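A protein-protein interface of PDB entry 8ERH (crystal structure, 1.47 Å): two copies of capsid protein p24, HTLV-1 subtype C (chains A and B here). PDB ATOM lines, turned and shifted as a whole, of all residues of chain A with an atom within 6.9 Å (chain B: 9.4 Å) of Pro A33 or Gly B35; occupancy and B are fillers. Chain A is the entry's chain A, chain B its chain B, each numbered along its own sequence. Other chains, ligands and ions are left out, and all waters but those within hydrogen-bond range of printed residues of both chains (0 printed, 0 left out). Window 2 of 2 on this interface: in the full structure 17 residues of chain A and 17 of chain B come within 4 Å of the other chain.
Pro A33 touches just these residues of chain B: Gly B35 and Thr B36. No residue of chain B comes within 4 Å of Leu A32. No residue of chain B comes within 4 Å of Gly A35. Thr A36 touches just these residues of chain B: Pro B33 (3.4 Å) and Thr B36 (2.8 Å). Printed residues of chain A within 4 Å of Pro B33: Thr A36 (3.4 Å). Of the printed residues of chain A, Thr B36 touches Pro A33 and Thr A36. Lys B38 touches none of the printed residues of chain A. The nearest residue of chain B that does not touch Pro A33 is Pro B37 (4.6 Å). The nearest residue of chain A that does not touch Gly B35 is Thr A36 (6.4 Å). The nearest printed residue of chain A that does not touch Ile B41 is Leu A32 (4.6 Å).
Pro A33 touches Gly B35, but with the chains exchanged Gly A35 does not touch Pro B33 (4.3 Å). Pro A33 touches Thr B36, and with the chains exchanged Thr A36 touches Pro B33. Thr A36 touches its own counterpart, Thr B36. Of the 6 pairs that touch across the chains among the printed residues, 3 have their exchanged pair printed and touching as well.
Trp A6 touches Pro B40 (CH2 to CB, 3.6 Å). Trp A6 touches Ile B41. Gly B35 touches Pro A33 (O to CG, 3.8 Å). Pro A33 touches Thr B36. Pro B33 touches Thr A36.
The side-chain hydroxyl (OG1) of Thr A36 sits at hydrogen-bond distance from the side-chain hydroxyl (OG1) of Thr B36 (2.8 Å).
Hydrophobic or aromatic side chains of chain B within 4 Å of the printed part of chain A: Pro B33, Pro B40 and Ile B41. Along chain B the printed residues that touch a printed residue of chain A span positions 33 to 41. Hydrophobic or aromatic side chains of chain A that line the printed part of chain B: Trp A6 and Pro A33.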
ATOM      1  N   TRP A   6     -20.564  20.686  32.771  1.00  0.00           N
ATOM      2  CA  TRP A   6     -20.690  21.847  33.645  1.00  0.00           C
ATOM      3  C   TRP A   6     -22.128  22.330  33.739  1.00  0.00           C
ATOM      4  O   TRP A   6     -22.476  22.989  34.720  1.00  0.00           O
ATOM      5  CB  TRP A   6     -19.738  22.982  33.223  1.00  0.00           C
ATOM      6  CG  TRP A   6     -19.971  23.623  31.864  1.00  0.00           C
ATOM      7  CD1 TRP A   6     -19.101  23.631  30.818  1.00  0.00           C
ATOM      8  CD2 TRP A   6     -21.103  24.420  31.445  1.00  0.00           C
ATOM      9  NE1 TRP A   6     -19.633  24.334  29.762  1.00  0.00           N
ATOM     10  CE2 TRP A   6     -20.855  24.829  30.120  1.00  0.00           C
ATOM     11  CE3 TRP A   6     -22.299  24.807  32.055  1.00  0.00           C
ATOM     12  CZ2 TRP A   6     -21.757  25.605  29.392  1.00  0.00           C
ATOM     13  CZ3 TRP A   6     -23.207  25.570  31.322  1.00  0.00           C
ATOM     14  CH2 TRP A   6     -22.923  25.964  30.009  1.00  0.00           C
ATOM     15  N   LEU A  28     -16.294  24.824  35.275  1.00  0.00           N
ATOM     16  CA  LEU A  28     -16.084  25.811  34.221  1.00  0.00           C
ATOM     17  C   LEU A  28     -14.602  25.999  33.917  1.00  0.00           C
ATOM     18  O   LEU A  28     -14.212  26.112  32.749  1.00  0.00           O
ATOM     19  CB  LEU A  28     -16.737  27.129  34.635  1.00  0.00           C
ATOM     20  CG  LEU A  28     -18.244  27.092  34.770  1.00  0.00           C
ATOM     21  CD1 LEU A  28     -18.791  28.378  35.403  1.00  0.00           C
ATOM     22  CD2 LEU A  28     -18.918  26.825  33.448  1.00  0.00           C
ATOM     23  N   ASP A  29     -13.756  26.020  34.951  1.00  0.00           N
ATOM     24  CA  ASP A  29     -12.318  26.097  34.731  1.00  0.00           C
ATOM     25  C   ASP A  29     -11.849  24.997  33.788  1.00  0.00           C
ATOM     26  O   ASP A  29     -11.003  25.234  32.916  1.00  0.00           O
ATOM     27  CB  ASP A  29     -11.582  25.992  36.067  1.00  0.00           C
ATOM     28  CG  ASP A  29     -11.498  27.312  36.797  1.00  0.00           C
ATOM     29  OD1 ASP A  29     -11.812  28.356  36.191  1.00  0.00           O
ATOM     30  OD2 ASP A  29     -11.099  27.312  37.981  1.00  0.00           O
ATOM     31  N   ASN A  30     -12.385  23.783  33.945  1.00  0.00           N
ATOM     32  CA  ASN A  30     -11.928  22.642  33.161  1.00  0.00           C
ATOM     33  C   ASN A  30     -12.773  22.369  31.926  1.00  0.00           C
ATOM     34  O   ASN A  30     -12.314  21.649  31.030  1.00  0.00           O
ATOM     35  CB  ASN A  30     -11.910  21.373  34.030  1.00  0.00           C
ATOM     36  CG  ASN A  30     -10.987  21.498  35.224  1.00  0.00           C
ATOM     37  OD1 ASN A  30      -9.944  22.150  35.152  1.00  0.00           O
ATOM     38  ND2 ASN A  30     -11.364  20.868  36.333  1.00  0.00           N
ATOM     39  N   GLY A  31     -13.973  22.930  31.843  1.00  0.00           N
ATOM     40  CA  GLY A  31     -14.877  22.627  30.754  1.00  0.00           C
ATOM     41  C   GLY A  31     -15.099  23.785  29.805  1.00  0.00           C
ATOM     42  O   GLY A  31     -15.026  23.612  28.587  1.00  0.00           O
ATOM     43  N   LEU A  32     -15.363  24.965  30.344  1.00  0.00           N
ATOM     44  CA  LEU A  32     -15.594  26.131  29.502  1.00  0.00           C
ATOM     45  C   LEU A  32     -14.363  26.391  28.644  1.00  0.00           C
ATOM     46  O   LEU A  32     -13.242  26.432  29.177  1.00  0.00           O
ATOM     47  CB  LEU A  32     -15.872  27.344  30.390  1.00  0.00           C
ATOM     48  CG  LEU A  32     -16.744  28.450  29.800  1.00  0.00           C
ATOM     49  CD1 LEU A  32     -18.114  27.928  29.415  1.00  0.00           C
ATOM     50  CD2 LEU A  32     -16.857  29.594  30.804  1.00  0.00           C
ATOM     51  N   PRO A  33     -14.518  26.561  27.327  1.00  0.00           N
ATOM     52  CA  PRO A  33     -13.349  26.816  26.479  1.00  0.00           C
ATOM     53  C   PRO A  33     -12.489  27.939  27.030  1.00  0.00           C
ATOM     54  O   PRO A  33     -12.989  28.949  27.525  1.00  0.00           O
ATOM     55  CB  PRO A  33     -13.966  27.194  25.128  1.00  0.00           C
ATOM     56  CG  PRO A  33     -15.280  26.472  25.108  1.00  0.00           C
ATOM     57  CD  PRO A  33     -15.760  26.431  26.535  1.00  0.00           C
ATOM     58  N   GLU A  34     -11.175  27.747  26.954  1.00  0.00           N
ATOM     59  CA  GLU A  34     -10.248  28.798  27.348  1.00  0.00           C
ATOM     60  C   GLU A  34     -10.517  30.043  26.515  1.00  0.00           C
ATOM     61  O   GLU A  34     -10.525  29.992  25.282  1.00  0.00           O
ATOM     62  CB  GLU A  34      -8.816  28.302  27.138  1.00  0.00           C
ATOM     63  CG  GLU A  34      -7.717  29.247  27.628  1.00  0.00           C
ATOM     64  CD  GLU A  34      -6.314  28.690  27.383  1.00  0.00           C
ATOM     65  OE1 GLU A  34      -6.205  27.612  26.758  1.00  0.00           O
ATOM     66  OE2 GLU A  34      -5.319  29.330  27.812  1.00  0.00           O
ATOM     67  N   GLY A  35     -10.741  31.162  27.193  1.00  0.00           N
ATOM     68  CA  GLY A  35     -10.983  32.431  26.546  1.00  0.00           C
ATOM     69  C   GLY A  35     -12.405  32.941  26.650  1.00  0.00           C
ATOM     70  O   GLY A  35     -12.635  34.138  26.430  1.00  0.00           O
ATOM     71  N   THR A  36     -13.362  32.079  26.956  1.00  0.00           N
ATOM     72  CA  THR A  36     -14.725  32.547  27.207  1.00  0.00           C
ATOM     73  C   THR A  36     -14.811  33.048  28.641  1.00  0.00           C
ATOM     74  O   THR A  36     -14.389  32.338  29.560  1.00  0.00           O
ATOM     75  CB  THR A  36     -15.714  31.403  27.005  1.00  0.00           C
ATOM     76  OG1 THR A  36     -15.790  31.077  25.609  1.00  0.00           O
ATOM     77  CG2 THR A  36     -17.096  31.789  27.521  1.00  0.00           C
ATOM     78  N   PRO A  37     -15.334  34.251  28.874  1.00  0.00           N
ATOM     79  CA  PRO A  37     -15.367  34.782  30.244  1.00  0.00           C
ATOM     80  C   PRO A  37     -16.165  33.880  31.168  1.00  0.00           C
ATOM     81  O   PRO A  37     -17.344  33.620  30.945  1.00  0.00           O
ATOM     82  CB  PRO A  37     -16.026  36.158  30.073  1.00  0.00           C
ATOM     83  CG  PRO A  37     -16.771  36.068  28.783  1.00  0.00           C
ATOM     84  CD  PRO A  37     -15.902  35.215  27.906  1.00  0.00           C
ATOM     85  N   LEU B  28     -25.745  36.071  22.024  1.00  0.00           N
ATOM     86  CA  LEU B  28     -24.827  34.964  22.257  1.00  0.00           C
ATOM     87  C   LEU B  28     -24.316  34.377  20.953  1.00  0.00           C
ATOM     88  O   LEU B  28     -23.116  34.083  20.833  1.00  0.00           O
ATOM     89  CB  LEU B  28     -25.523  33.881  23.081  1.00  0.00           C
ATOM     90  CG  LEU B  28     -25.916  34.292  24.496  1.00  0.00           C
ATOM     91  CD1 LEU B  28     -26.916  33.277  25.113  1.00  0.00           C
ATOM     92  CD2 LEU B  28     -24.662  34.405  25.369  1.00  0.00           C
ATOM     93  N   ASP B  29     -25.199  34.216  19.957  1.00  0.00           N
ATOM     94  CA  ASP B  29     -24.764  33.815  18.620  1.00  0.00           C
ATOM     95  C   ASP B  29     -23.610  34.695  18.146  1.00  0.00           C
ATOM     96  O   ASP B  29     -22.615  34.212  17.595  1.00  0.00           O
ATOM     97  CB  ASP B  29     -25.927  33.977  17.632  1.00  0.00           C
ATOM     98  CG  ASP B  29     -26.799  32.749  17.513  1.00  0.00           C
ATOM     99  OD1 ASP B  29     -26.431  31.694  18.050  1.00  0.00           O
ATOM    100  OD2 ASP B  29     -27.872  32.849  16.872  1.00  0.00           O
ATOM    101  N   GLY B  31     -21.731  37.003  19.978  1.00  0.00           N
ATOM    102  CA  GLY B  31     -20.742  37.462  20.933  1.00  0.00           C
ATOM    103  C   GLY B  31     -19.975  36.373  21.660  1.00  0.00           C
ATOM    104  O   GLY B  31     -18.846  36.614  22.097  1.00  0.00           O
ATOM    105  N   LEU B  32     -20.532  35.180  21.765  1.00  0.00           N
ATOM    106  CA  LEU B  32     -19.768  34.087  22.354  1.00  0.00           C
ATOM    107  C   LEU B  32     -18.622  33.709  21.418  1.00  0.00           C
ATOM    108  O   LEU B  32     -18.791  33.707  20.190  1.00  0.00           O
ATOM    109  CB  LEU B  32     -20.656  32.874  22.566  1.00  0.00           C
ATOM    110  CG  LEU B  32     -21.541  32.881  23.803  1.00  0.00           C
ATOM    111  CD1 LEU B  32     -22.441  31.649  23.779  1.00  0.00           C
ATOM    112  CD2 LEU B  32     -20.735  32.931  25.097  1.00  0.00           C
ATOM    113  N   PRO B  33     -17.444  33.393  21.954  1.00  0.00           N
ATOM    114  CA  PRO B  33     -16.331  32.987  21.087  1.00  0.00           C
ATOM    115  C   PRO B  33     -16.680  31.778  20.234  1.00  0.00           C
ATOM    116  O   PRO B  33     -17.550  30.977  20.571  1.00  0.00           O
ATOM    117  CB  PRO B  33     -15.209  32.649  22.082  1.00  0.00           C
ATOM    118  CG  PRO B  33     -15.509  33.505  23.268  1.00  0.00           C
ATOM    119  CD  PRO B  33     -17.025  33.521  23.362  1.00  0.00           C
ATOM    120  N   GLU B  34     -15.972  31.643  19.106  1.00  0.00           N
ATOM    121  CA  GLU B  34     -16.133  30.447  18.288  1.00  0.00           C
ATOM    122  C   GLU B  34     -15.924  29.195  19.127  1.00  0.00           C
ATOM    123  O   GLU B  34     -15.035  29.139  19.982  1.00  0.00           O
ATOM    124  CB  GLU B  34     -15.112  30.420  17.148  1.00  0.00           C
ATOM    125  CG  GLU B  34     -15.054  31.636  16.287  1.00  0.00           C
ATOM    126  CD  GLU B  34     -13.891  31.567  15.311  1.00  0.00           C
ATOM    127  OE1 GLU B  34     -13.870  30.609  14.491  1.00  0.00           O
ATOM    128  OE2 GLU B  34     -13.006  32.454  15.371  1.00  0.00           O
ATOM    129  N   GLY B  35     -16.727  28.170  18.856  1.00  0.00           N
ATOM    130  CA  GLY B  35     -16.553  26.893  19.504  1.00  0.00           C
ATOM    131  C   GLY B  35     -17.031  26.818  20.932  1.00  0.00           C
ATOM    132  O   GLY B  35     -16.741  25.828  21.613  1.00  0.00           O
ATOM    133  N   THR B  36     -17.739  27.841  21.418  1.00  0.00           N
ATOM    134  CA  THR B  36     -18.383  27.748  22.723  1.00  0.00           C
ATOM    135  C   THR B  36     -19.844  27.384  22.525  1.00  0.00           C
ATOM    136  O   THR B  36     -20.542  28.070  21.762  1.00  0.00           O
ATOM    137  CB  THR B  36     -18.280  29.079  23.461  1.00  0.00           C
ATOM    138  OG1 THR B  36     -16.900  29.415  23.663  1.00  0.00           O
ATOM    139  CG2 THR B  36     -18.973  28.994  24.823  1.00  0.00           C
ATOM    140  N   PRO B  37     -20.349  26.330  23.169  1.00  0.00           N
ATOM    141  CA  PRO B  37     -21.735  25.904  22.907  1.00  0.00           C
ATOM    142  C   PRO B  37     -22.725  26.933  23.429  1.00  0.00           C
ATOM    143  O   PRO B  37     -22.725  27.259  24.617  1.00  0.00           O
ATOM    144  CB  PRO B  37     -21.861  24.571  23.653  1.00  0.00           C
ATOM    145  CG  PRO B  37     -20.680  24.468  24.553  1.00  0.00           C
ATOM    146  CD  PRO B  37     -19.683  25.536  24.220  1.00  0.00           C
ATOM    147  N   LYS B  38     -23.580  27.429  22.531  1.00  0.00           N
ATOM    148  CA  LYS B  38     -24.539  28.463  22.907  1.00  0.00           C
ATOM    149  C   LYS B  38     -25.681  27.911  23.752  1.00  0.00           C
ATOM    150  O   LYS B  38     -26.109  28.557  24.716  1.00  0.00           O
ATOM    151  CB  LYS B  38     -25.107  29.121  21.653  1.00  0.00           C
ATOM    152  CG  LYS B  38     -26.297  30.015  21.923  1.00  0.00           C
ATOM    153  CD  LYS B  38     -26.871  30.593  20.637  1.00  0.00           C
ATOM    154  CE  LYS B  38     -27.392  29.493  19.736  1.00  0.00           C
ATOM    155  NZ  LYS B  38     -28.457  29.955  18.826  1.00  0.00           N
ATOM    156  N   PRO B  40     -26.574  25.646  26.161  1.00  0.00           N
ATOM    157  CA  PRO B  40     -26.663  25.617  27.632  1.00  0.00           C
ATOM    158  C   PRO B  40     -26.460  26.981  28.276  1.00  0.00           C
ATOM    159  O   PRO B  40     -27.026  27.246  29.347  1.00  0.00           O
ATOM    160  CB  PRO B  40     -25.578  24.603  28.038  1.00  0.00           C
ATOM    161  CG  PRO B  40     -24.619  24.592  26.892  1.00  0.00           C
ATOM    162  CD  PRO B  40     -25.440  24.852  25.646  1.00  0.00           C
ATOM    163  N   ILE B  41     -25.662  27.853  27.661  1.00  0.00           N
ATOM    164  CA  ILE B  41     -25.481  29.189  28.208  1.00  0.00           C
ATOM    165  C   ILE B  41     -26.758  29.997  28.026  1.00  0.00           C
ATOM    166  O   ILE B  41     -27.204  30.714  28.938  1.00  0.00           O
ATOM    167  CB  ILE B  41     -24.246  29.841  27.552  1.00  0.00           C
ATOM    168  CG1 ILE B  41     -22.978  29.082  27.971  1.00  0.00           C
ATOM    169  CG2 ILE B  41     -24.143  31.319  27.911  1.00  0.00           C
ATOM    170  CD1 ILE B  41     -21.770  29.375  27.100  1.00  0.00           C
